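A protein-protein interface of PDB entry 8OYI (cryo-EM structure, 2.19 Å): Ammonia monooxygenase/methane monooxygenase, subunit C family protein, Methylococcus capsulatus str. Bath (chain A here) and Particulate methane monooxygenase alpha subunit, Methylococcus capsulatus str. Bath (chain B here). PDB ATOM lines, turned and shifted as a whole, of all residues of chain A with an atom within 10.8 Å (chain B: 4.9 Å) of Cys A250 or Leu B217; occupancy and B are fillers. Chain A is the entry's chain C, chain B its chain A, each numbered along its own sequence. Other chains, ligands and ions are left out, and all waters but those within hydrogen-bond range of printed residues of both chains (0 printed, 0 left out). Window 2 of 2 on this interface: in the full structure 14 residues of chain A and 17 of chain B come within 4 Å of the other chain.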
ATOM      1  N   LEU A 233      20.419  10.797  -2.927  1.00  0.00           N
ATOM      2  CA  LEU A 233      19.356  10.881  -1.937  1.00  0.00           C
ATOM      3  C   LEU A 233      18.306  11.910  -2.325  1.00  0.00           C
ATOM      4  O   LEU A 233      17.121  11.718  -2.042  1.00  0.00           O
ATOM      5  CB  LEU A 233      19.933  11.195  -0.561  1.00  0.00           C
ATOM      6  CG  LEU A 233      20.002   9.964   0.340  1.00  0.00           C
ATOM      7  CD1 LEU A 233      20.577  10.324   1.685  1.00  0.00           C
ATOM      8  CD2 LEU A 233      18.627   9.340   0.504  1.00  0.00           C
ATOM      9  N   THR A 234      18.700  13.017  -2.963  1.00  0.00           N
ATOM     10  CA  THR A 234      17.648  13.902  -3.459  1.00  0.00           C
ATOM     11  C   THR A 234      16.868  13.241  -4.590  1.00  0.00           C
ATOM     12  O   THR A 234      15.651  13.449  -4.709  1.00  0.00           O
ATOM     13  CB  THR A 234      18.214  15.258  -3.891  1.00  0.00           C
ATOM     14  OG1 THR A 234      17.182  16.030  -4.519  1.00  0.00           O
ATOM     15  CG2 THR A 234      19.347  15.099  -4.852  1.00  0.00           C
ATOM     16  N   GLN A 235      17.527  12.403  -5.396  1.00  0.00           N
ATOM     17  CA  GLN A 235      16.801  11.617  -6.392  1.00  0.00           C
ATOM     18  C   GLN A 235      15.817  10.652  -5.734  1.00  0.00           C
ATOM     19  O   GLN A 235      14.677  10.517  -6.191  1.00  0.00           O
ATOM     20  CB  GLN A 235      17.786  10.862  -7.278  1.00  0.00           C
ATOM     21  CG  GLN A 235      18.225  11.629  -8.510  1.00  0.00           C
ATOM     22  CD  GLN A 235      19.200  10.841  -9.354  1.00  0.00           C
ATOM     23  OE1 GLN A 235      19.563   9.720  -9.007  1.00  0.00           O
ATOM     24  NE2 GLN A 235      19.628  11.421 -10.468  1.00  0.00           N
ATOM     25  N   THR A 236      16.240   9.971  -4.664  1.00  0.00           N
ATOM     26  CA  THR A 236      15.318   9.077  -3.963  1.00  0.00           C
ATOM     27  C   THR A 236      14.196   9.843  -3.281  1.00  0.00           C
ATOM     28  O   THR A 236      13.084   9.325  -3.162  1.00  0.00           O
ATOM     29  CB  THR A 236      16.041   8.210  -2.925  1.00  0.00           C
ATOM     30  OG1 THR A 236      16.292   8.978  -1.740  1.00  0.00           O
ATOM     31  CG2 THR A 236      17.327   7.637  -3.467  1.00  0.00           C
ATOM     32  N   PHE A 237      14.462  11.060  -2.810  1.00  0.00           N
ATOM     33  CA  PHE A 237      13.401  11.884  -2.244  1.00  0.00           C
ATOM     34  C   PHE A 237      12.359  12.223  -3.302  1.00  0.00           C
ATOM     35  O   PHE A 237      11.151  12.146  -3.051  1.00  0.00           O
ATOM     36  CB  PHE A 237      13.989  13.158  -1.640  1.00  0.00           C
ATOM     37  CG  PHE A 237      14.757  12.929  -0.377  1.00  0.00           C
ATOM     38  CD1 PHE A 237      14.511  11.820   0.409  1.00  0.00           C
ATOM     39  CD2 PHE A 237      15.735  13.824   0.023  1.00  0.00           C
ATOM     40  CE1 PHE A 237      15.221  11.606   1.570  1.00  0.00           C
ATOM     41  CE2 PHE A 237      16.449  13.616   1.182  1.00  0.00           C
ATOM     42  CZ  PHE A 237      16.193  12.507   1.955  1.00  0.00           C
ATOM     43  N   TYR A 238      12.816  12.600  -4.497  1.00  0.00           N
ATOM     44  CA  TYR A 238      11.883  12.866  -5.587  1.00  0.00           C
ATOM     45  C   TYR A 238      11.113  11.611  -5.976  1.00  0.00           C
ATOM     46  O   TYR A 238       9.913  11.673  -6.271  1.00  0.00           O
ATOM     47  CB  TYR A 238      12.628  13.441  -6.793  1.00  0.00           C
ATOM     48  CG  TYR A 238      13.020  14.886  -6.620  1.00  0.00           C
ATOM     49  CD1 TYR A 238      12.192  15.774  -5.948  1.00  0.00           C
ATOM     50  CD2 TYR A 238      14.217  15.364  -7.133  1.00  0.00           C
ATOM     51  CE1 TYR A 238      12.544  17.099  -5.787  1.00  0.00           C
ATOM     52  CE2 TYR A 238      14.580  16.688  -6.977  1.00  0.00           C
ATOM     53  CZ  TYR A 238      13.740  17.548  -6.303  1.00  0.00           C
ATOM     54  OH  TYR A 238      14.099  18.866  -6.149  1.00  0.00           O
ATOM     55  N   SER A 239      11.787  10.458  -5.986  1.00  0.00           N
ATOM     56  CA  SER A 239      11.109   9.201  -6.289  1.00  0.00           C
ATOM     57  C   SER A 239      10.066   8.860  -5.234  1.00  0.00           C
ATOM     58  O   SER A 239       8.989   8.352  -5.568  1.00  0.00           O
ATOM     59  CB  SER A 239      12.134   8.074  -6.410  1.00  0.00           C
ATOM     60  OG  SER A 239      11.590   6.839  -5.984  1.00  0.00           O
ATOM     61  N   PHE A 240      10.374   9.114  -3.963  1.00  0.00           N
ATOM     62  CA  PHE A 240       9.398   8.950  -2.894  1.00  0.00           C
ATOM     63  C   PHE A 240       8.200   9.863  -3.104  1.00  0.00           C
ATOM     64  O   PHE A 240       7.049   9.440  -2.951  1.00  0.00           O
ATOM     65  CB  PHE A 240      10.055   9.251  -1.547  1.00  0.00           C
ATOM     66  CG  PHE A 240      10.414   8.034  -0.748  1.00  0.00           C
ATOM     67  CD1 PHE A 240       9.432   7.268  -0.147  1.00  0.00           C
ATOM     68  CD2 PHE A 240      11.739   7.668  -0.579  1.00  0.00           C
ATOM     69  CE1 PHE A 240       9.762   6.155   0.602  1.00  0.00           C
ATOM     70  CE2 PHE A 240      12.075   6.554   0.162  1.00  0.00           C
ATOM     71  CZ  PHE A 240      11.086   5.798   0.754  1.00  0.00           C
ATOM     72  N   ALA A 241       8.455  11.117  -3.457  1.00  0.00           N
ATOM     73  CA  ALA A 241       7.411  12.123  -3.635  1.00  0.00           C
ATOM     74  C   ALA A 241       6.944  12.199  -5.083  1.00  0.00           C
ATOM     75  O   ALA A 241       6.918  13.274  -5.682  1.00  0.00           O
ATOM     76  CB  ALA A 241       7.916  13.478  -3.153  1.00  0.00           C
ATOM     77  N   GLN A 242       6.567  11.064  -5.669  1.00  0.00           N
ATOM     78  CA  GLN A 242       6.082  11.053  -7.056  1.00  0.00           C
ATOM     79  C   GLN A 242       4.558  11.117  -7.089  1.00  0.00           C
ATOM     80  O   GLN A 242       3.979  12.099  -7.564  1.00  0.00           O
ATOM     81  CB  GLN A 242       6.593   9.808  -7.785  1.00  0.00           C
ATOM     82  CG  GLN A 242       8.012   9.910  -8.343  1.00  0.00           C
ATOM     83  CD  GLN A 242       8.144  10.903  -9.487  1.00  0.00           C
ATOM     84  OE1 GLN A 242       7.817  12.083  -9.353  1.00  0.00           O
ATOM     85  NE2 GLN A 242       8.626  10.419 -10.627  1.00  0.00           N
ATOM     86  N   GLY A 243       3.899  10.080  -6.585  1.00  0.00           N
ATOM     87  CA  GLY A 243       2.452  10.074  -6.494  1.00  0.00           C
ATOM     88  C   GLY A 243       1.961  10.251  -5.078  1.00  0.00           C
ATOM     89  O   GLY A 243       0.997  10.983  -4.823  1.00  0.00           O
ATOM     90  N   GLY A 244       2.630   9.590  -4.139  1.00  0.00           N
ATOM     91  CA  GLY A 244       2.279   9.683  -2.738  1.00  0.00           C
ATOM     92  C   GLY A 244       3.096  10.723  -2.003  1.00  0.00           C
ATOM     93  O   GLY A 244       3.468  10.523  -0.843  1.00  0.00           O
ATOM     94  N   LEU A 245       3.395  11.835  -2.675  1.00  0.00           N
ATOM     95  CA  LEU A 245       4.117  12.925  -2.035  1.00  0.00           C
ATOM     96  C   LEU A 245       3.349  13.502  -0.858  1.00  0.00           C
ATOM     97  O   LEU A 245       3.958  14.124   0.021  1.00  0.00           O
ATOM     98  CB  LEU A 245       4.424  14.023  -3.061  1.00  0.00           C
ATOM     99  CG  LEU A 245       3.384  15.074  -3.457  1.00  0.00           C
ATOM    100  CD1 LEU A 245       3.468  16.309  -2.566  1.00  0.00           C
ATOM    101  CD2 LEU A 245       3.539  15.454  -4.922  1.00  0.00           C
ATOM    102  N   GLY A 246       2.033  13.316  -0.825  1.00  0.00           N
ATOM    103  CA  GLY A 246       1.218  13.769   0.276  1.00  0.00           C
ATOM    104  C   GLY A 246      -0.226  13.368   0.072  1.00  0.00           C
ATOM    105  O   GLY A 246      -0.528  12.273  -0.409  1.00  0.00           O
ATOM    106  N   GLN A 247      -1.119  14.286   0.410  1.00  0.00           N
ATOM    107  CA  GLN A 247      -0.703  15.621   0.817  1.00  0.00           C
ATOM    108  C   GLN A 247      -0.633  15.768   2.329  1.00  0.00           C
ATOM    109  O   GLN A 247      -0.997  14.848   3.066  1.00  0.00           O
ATOM    110  CB  GLN A 247      -1.639  16.671   0.226  1.00  0.00           C
ATOM    111  CG  GLN A 247      -1.546  16.779  -1.287  1.00  0.00           C
ATOM    112  CD  GLN A 247      -0.117  16.703  -1.787  1.00  0.00           C
ATOM    113  OE1 GLN A 247       0.317  15.674  -2.301  1.00  0.00           O
ATOM    114  NE2 GLN A 247       0.623  17.795  -1.633  1.00  0.00           N
ATOM    115  N   SER A 248      -0.240  16.979   2.744  1.00  0.00           N
ATOM    116  CA  SER A 248       0.352  17.331   4.033  1.00  0.00           C
ATOM    117  C   SER A 248       1.581  18.173   3.736  1.00  0.00           C
ATOM    118  O   SER A 248       1.579  19.393   3.928  1.00  0.00           O
ATOM    119  CB  SER A 248       0.759  16.114   4.867  1.00  0.00           C
ATOM    120  OG  SER A 248       1.717  16.467   5.849  1.00  0.00           O
ATOM    121  N   LEU A 249       2.639  17.507   3.282  1.00  0.00           N
ATOM    122  CA  LEU A 249       3.818  18.179   2.755  1.00  0.00           C
ATOM    123  C   LEU A 249       3.415  19.165   1.671  1.00  0.00           C
ATOM    124  O   LEU A 249       2.765  18.791   0.688  1.00  0.00           O
ATOM    125  CB  LEU A 249       4.802  17.144   2.197  1.00  0.00           C
ATOM    126  CG  LEU A 249       5.535  16.128   3.090  1.00  0.00           C
ATOM    127  CD1 LEU A 249       4.630  15.336   4.027  1.00  0.00           C
ATOM    128  CD2 LEU A 249       6.311  15.171   2.213  1.00  0.00           C
ATOM    129  N   CYS A 250       3.795  20.431   1.860  1.00  0.00           N
ATOM    130  CA  CYS A 250       3.404  21.522   0.966  1.00  0.00           C
ATOM    131  C   CYS A 250       1.884  21.629   0.863  1.00  0.00           C
ATOM    132  O   CYS A 250       1.324  21.944  -0.193  1.00  0.00           O
ATOM    133  CB  CYS A 250       4.042  21.363  -0.415  1.00  0.00           C
ATOM    134  SG  CYS A 250       5.661  22.150  -0.583  1.00  0.00           S
ATOM    135  N   GLU A 251       1.212  21.364   1.982  1.00  0.00           N
ATOM    136  CA  GLU A 251      -0.230  21.553   2.090  1.00  0.00           C
ATOM    137  C   GLU A 251      -0.653  21.604   3.553  1.00  0.00           C
ATOM    138  O   GLU A 251      -0.555  22.646   4.202  1.00  0.00           O
ATOM    139  CB  GLU A 251      -0.998  20.442   1.368  1.00  0.00           C
ATOM    140  CG  GLU A 251      -2.278  20.935   0.705  1.00  0.00           C
ATOM    141  CD  GLU A 251      -2.871  19.931  -0.264  1.00  0.00           C
ATOM    142  OE1 GLU A 251      -3.636  19.053   0.189  1.00  0.00           O
ATOM    143  OE2 GLU A 251      -2.571  20.015  -1.473  1.00  0.00           O
ATOM    144  N   ILE B 213      12.296  15.795   3.433  1.00  0.00           N
ATOM    145  CA  ILE B 213      11.433  15.902   2.258  1.00  0.00           C
ATOM    146  C   ILE B 213      10.563  17.156   2.321  1.00  0.00           C
ATOM    147  O   ILE B 213      10.484  17.881   1.318  1.00  0.00           O
ATOM    148  CB  ILE B 213      10.581  14.635   2.069  1.00  0.00           C
ATOM    149  CG1 ILE B 213      11.473  13.450   1.691  1.00  0.00           C
ATOM    150  CG2 ILE B 213       9.560  14.856   0.973  1.00  0.00           C
ATOM    151  CD1 ILE B 213      10.722  12.279   1.095  1.00  0.00           C
ATOM    152  N   PRO B 214       9.870  17.450   3.430  1.00  0.00           N
ATOM    153  CA  PRO B 214       9.121  18.718   3.472  1.00  0.00           C
ATOM    154  C   PRO B 214      10.000  19.945   3.312  1.00  0.00           C
ATOM    155  O   PRO B 214       9.597  20.901   2.643  1.00  0.00           O
ATOM    156  CB  PRO B 214       8.436  18.677   4.847  1.00  0.00           C
ATOM    157  CG  PRO B 214       9.201  17.690   5.633  1.00  0.00           C
ATOM    158  CD  PRO B 214       9.654  16.664   4.659  1.00  0.00           C
ATOM    159  N   ARG B 215      11.206  19.941   3.887  1.00  0.00           N
ATOM    160  CA  ARG B 215      12.100  21.085   3.715  1.00  0.00           C
ATOM    161  C   ARG B 215      12.569  21.202   2.272  1.00  0.00           C
ATOM    162  O   ARG B 215      12.663  22.309   1.732  1.00  0.00           O
ATOM    163  CB  ARG B 215      13.293  20.982   4.667  1.00  0.00           C
ATOM    164  CG  ARG B 215      12.948  21.242   6.123  1.00  0.00           C
ATOM    165  CD  ARG B 215      14.178  21.225   7.009  1.00  0.00           C
ATOM    166  NE  ARG B 215      14.853  22.515   7.043  1.00  0.00           N
ATOM    167  CZ  ARG B 215      14.624  23.455   7.949  1.00  0.00           C
ATOM    168  NH1 ARG B 215      13.726  23.289   8.906  1.00  0.00           N
ATOM    169  NH2 ARG B 215      15.315  24.590   7.894  1.00  0.00           N
ATOM    170  N   LEU B 216      12.863  20.068   1.631  1.00  0.00           N
ATOM    171  CA  LEU B 216      13.239  20.085   0.222  1.00  0.00           C
ATOM    172  C   LEU B 216      12.111  20.645  -0.637  1.00  0.00           C
ATOM    173  O   LEU B 216      12.350  21.464  -1.533  1.00  0.00           O
ATOM    174  CB  LEU B 216      13.603  18.674  -0.232  1.00  0.00           C
ATOM    175  CG  LEU B 216      13.813  18.430  -1.725  1.00  0.00           C
ATOM    176  CD1 LEU B 216      15.102  19.081  -2.194  1.00  0.00           C
ATOM    177  CD2 LEU B 216      13.819  16.940  -2.028  1.00  0.00           C
ATOM    178  N   LEU B 217      10.877  20.214  -0.370  1.00  0.00           N
ATOM    179  CA  LEU B 217       9.737  20.712  -1.131  1.00  0.00           C
ATOM    180  C   LEU B 217       9.519  22.202  -0.895  1.00  0.00           C
ATOM    181  O   LEU B 217       9.190  22.940  -1.829  1.00  0.00           O
ATOM    182  CB  LEU B 217       8.478  19.923  -0.769  1.00  0.00           C
ATOM    183  CG  LEU B 217       8.425  18.477  -1.259  1.00  0.00           C
ATOM    184  CD1 LEU B 217       7.214  17.762  -0.686  1.00  0.00           C
ATOM    185  CD2 LEU B 217       8.416  18.421  -2.775  1.00  0.00           C
ATOM    186  N   MET B 218       9.687  22.658   0.347  1.00  0.00           N
ATOM    187  CA  MET B 218       9.538  24.081   0.636  1.00  0.00           C
ATOM    188  C   MET B 218      10.597  24.907  -0.081  1.00  0.00           C
ATOM    189  O   MET B 218      10.295  25.981  -0.613  1.00  0.00           O
ATOM    190  CB  MET B 218       9.604  24.321   2.143  1.00  0.00           C
ATOM    191  CG  MET B 218       8.346  23.912   2.889  1.00  0.00           C
ATOM    192  SD  MET B 218       7.023  25.115   2.706  1.00  0.00           S
ATOM    193  CE  MET B 218       7.719  26.512   3.583  1.00  0.00           C
ATOM    194  N   VAL B 219      11.841  24.427  -0.100  1.00  0.00           N
ATOM    195  CA  VAL B 219      12.904  25.161  -0.780  1.00  0.00           C
ATOM    196  C   VAL B 219      12.666  25.186  -2.286  1.00  0.00           C
ATOM    197  O   VAL B 219      12.849  26.220  -2.939  1.00  0.00           O
ATOM    198  CB  VAL B 219      14.279  24.565  -0.431  1.00  0.00           C
ATOM    199  CG1 VAL B 219      15.361  25.175  -1.305  1.00  0.00           C
ATOM    200  CG2 VAL B 219      14.597  24.792   1.039  1.00  0.00           C
ATOM    201  N   ASP B 220      12.246  24.054  -2.861  1.00  0.00           N
ATOM    202  CA  ASP B 220      12.042  23.983  -4.308  1.00  0.00           C
ATOM    203  C   ASP B 220      10.841  24.817  -4.745  1.00  0.00           C
ATOM    204  O   ASP B 220      10.964  25.728  -5.570  1.00  0.00           O
ATOM    205  CB  ASP B 220      11.873  22.524  -4.743  1.00  0.00           C
ATOM    206  CG  ASP B 220      13.171  21.744  -4.680  1.00  0.00           C
ATOM    207  OD1 ASP B 220      14.234  22.324  -4.988  1.00  0.00           O
ATOM    208  OD2 ASP B 220      13.129  20.547  -4.328  1.00  0.00           O
ATOM    209  N   ALA B 221       9.664  24.515  -4.198  1.00  0.00           N
ATOM    210  CA  ALA B 221       8.441  25.200  -4.597  1.00  0.00           C
ATOM    211  C   ALA B 221       8.386  26.593  -3.990  1.00  0.00           C
ATOM    212  O   ALA B 221       7.919  26.770  -2.861  1.00  0.00           O
ATOM    213  CB  ALA B 221       7.212  24.390  -4.185  1.00  0.00           C
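The side-chain carboxylate (OD2) of Asp B220 lies within hydrogen-bond range of the side-chain hydroxyl (OH) of Tyr A238 (2.7 Å).
NE2 of Gln A247 is in hydrogen-bond range of O of Leu A249 (3.3 Å).
Among the printed residues, merely in contact across the chains: Leu A249 with Ile B213 (3.5 Å), Cys A250 with Leu B217 (3.6 Å), Phe A237 with Ile B213 (3.7 Å), Phe A237 with Leu B216 (3.8 Å), Leu A249 with Leu B217 (3.8 Å) and Tyr A238 with Leu B216 (3.97 Å).
Gln A235 touches none of the printed residues of chain B. Of the printed residues of chain B, Phe A237 touches Ile B213 and Leu B216. Of the printed residues of chain B, Tyr A238 touches Leu B216 and Asp B220. Ser A239 touches none of the printed residues of chain B. Printed residues of chain B within 4 Å of Leu A249: Ile B213 (3.5 Å) and Leu B217 (3.8 Å). Cys A250 touches just one residue of chain B: Leu B217. Ile B213 touches just these residues of chain A: Phe A237 and Leu A249. No residue of chain A comes within 4 Å of Pro B214. Of chain A, only Phe A237 (3.8 Å) and Tyr A238 (3.97 Å) come within 4 Å of Leu B216. Leu B217 touches just these residues of chain A: Leu A249 (3.8 Å) and Cys A250 (3.6 Å). No residue of chain A comes within 4 Å of Val B219. Of chain A, only Tyr A238 (2.7 Å) comes within 4 Å of Asp B220. The nearest residue of chain B that does not touch Cys A250 is Met B218 (4.2 Å). The nearest residue of chain A that does not touch Leu B217 is Leu A245 (4.4 Å). The nearest printed residue of chain B that does not touch Tyr A238 is Leu B217 (5.3 Å).
Hydrophobic or aromatic side chains of chain B within 4 Å of the printed part of chain A: Ile B213, Leu B216 and Leu B217. Among the printed residues, 7 pairs touch across the chains.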
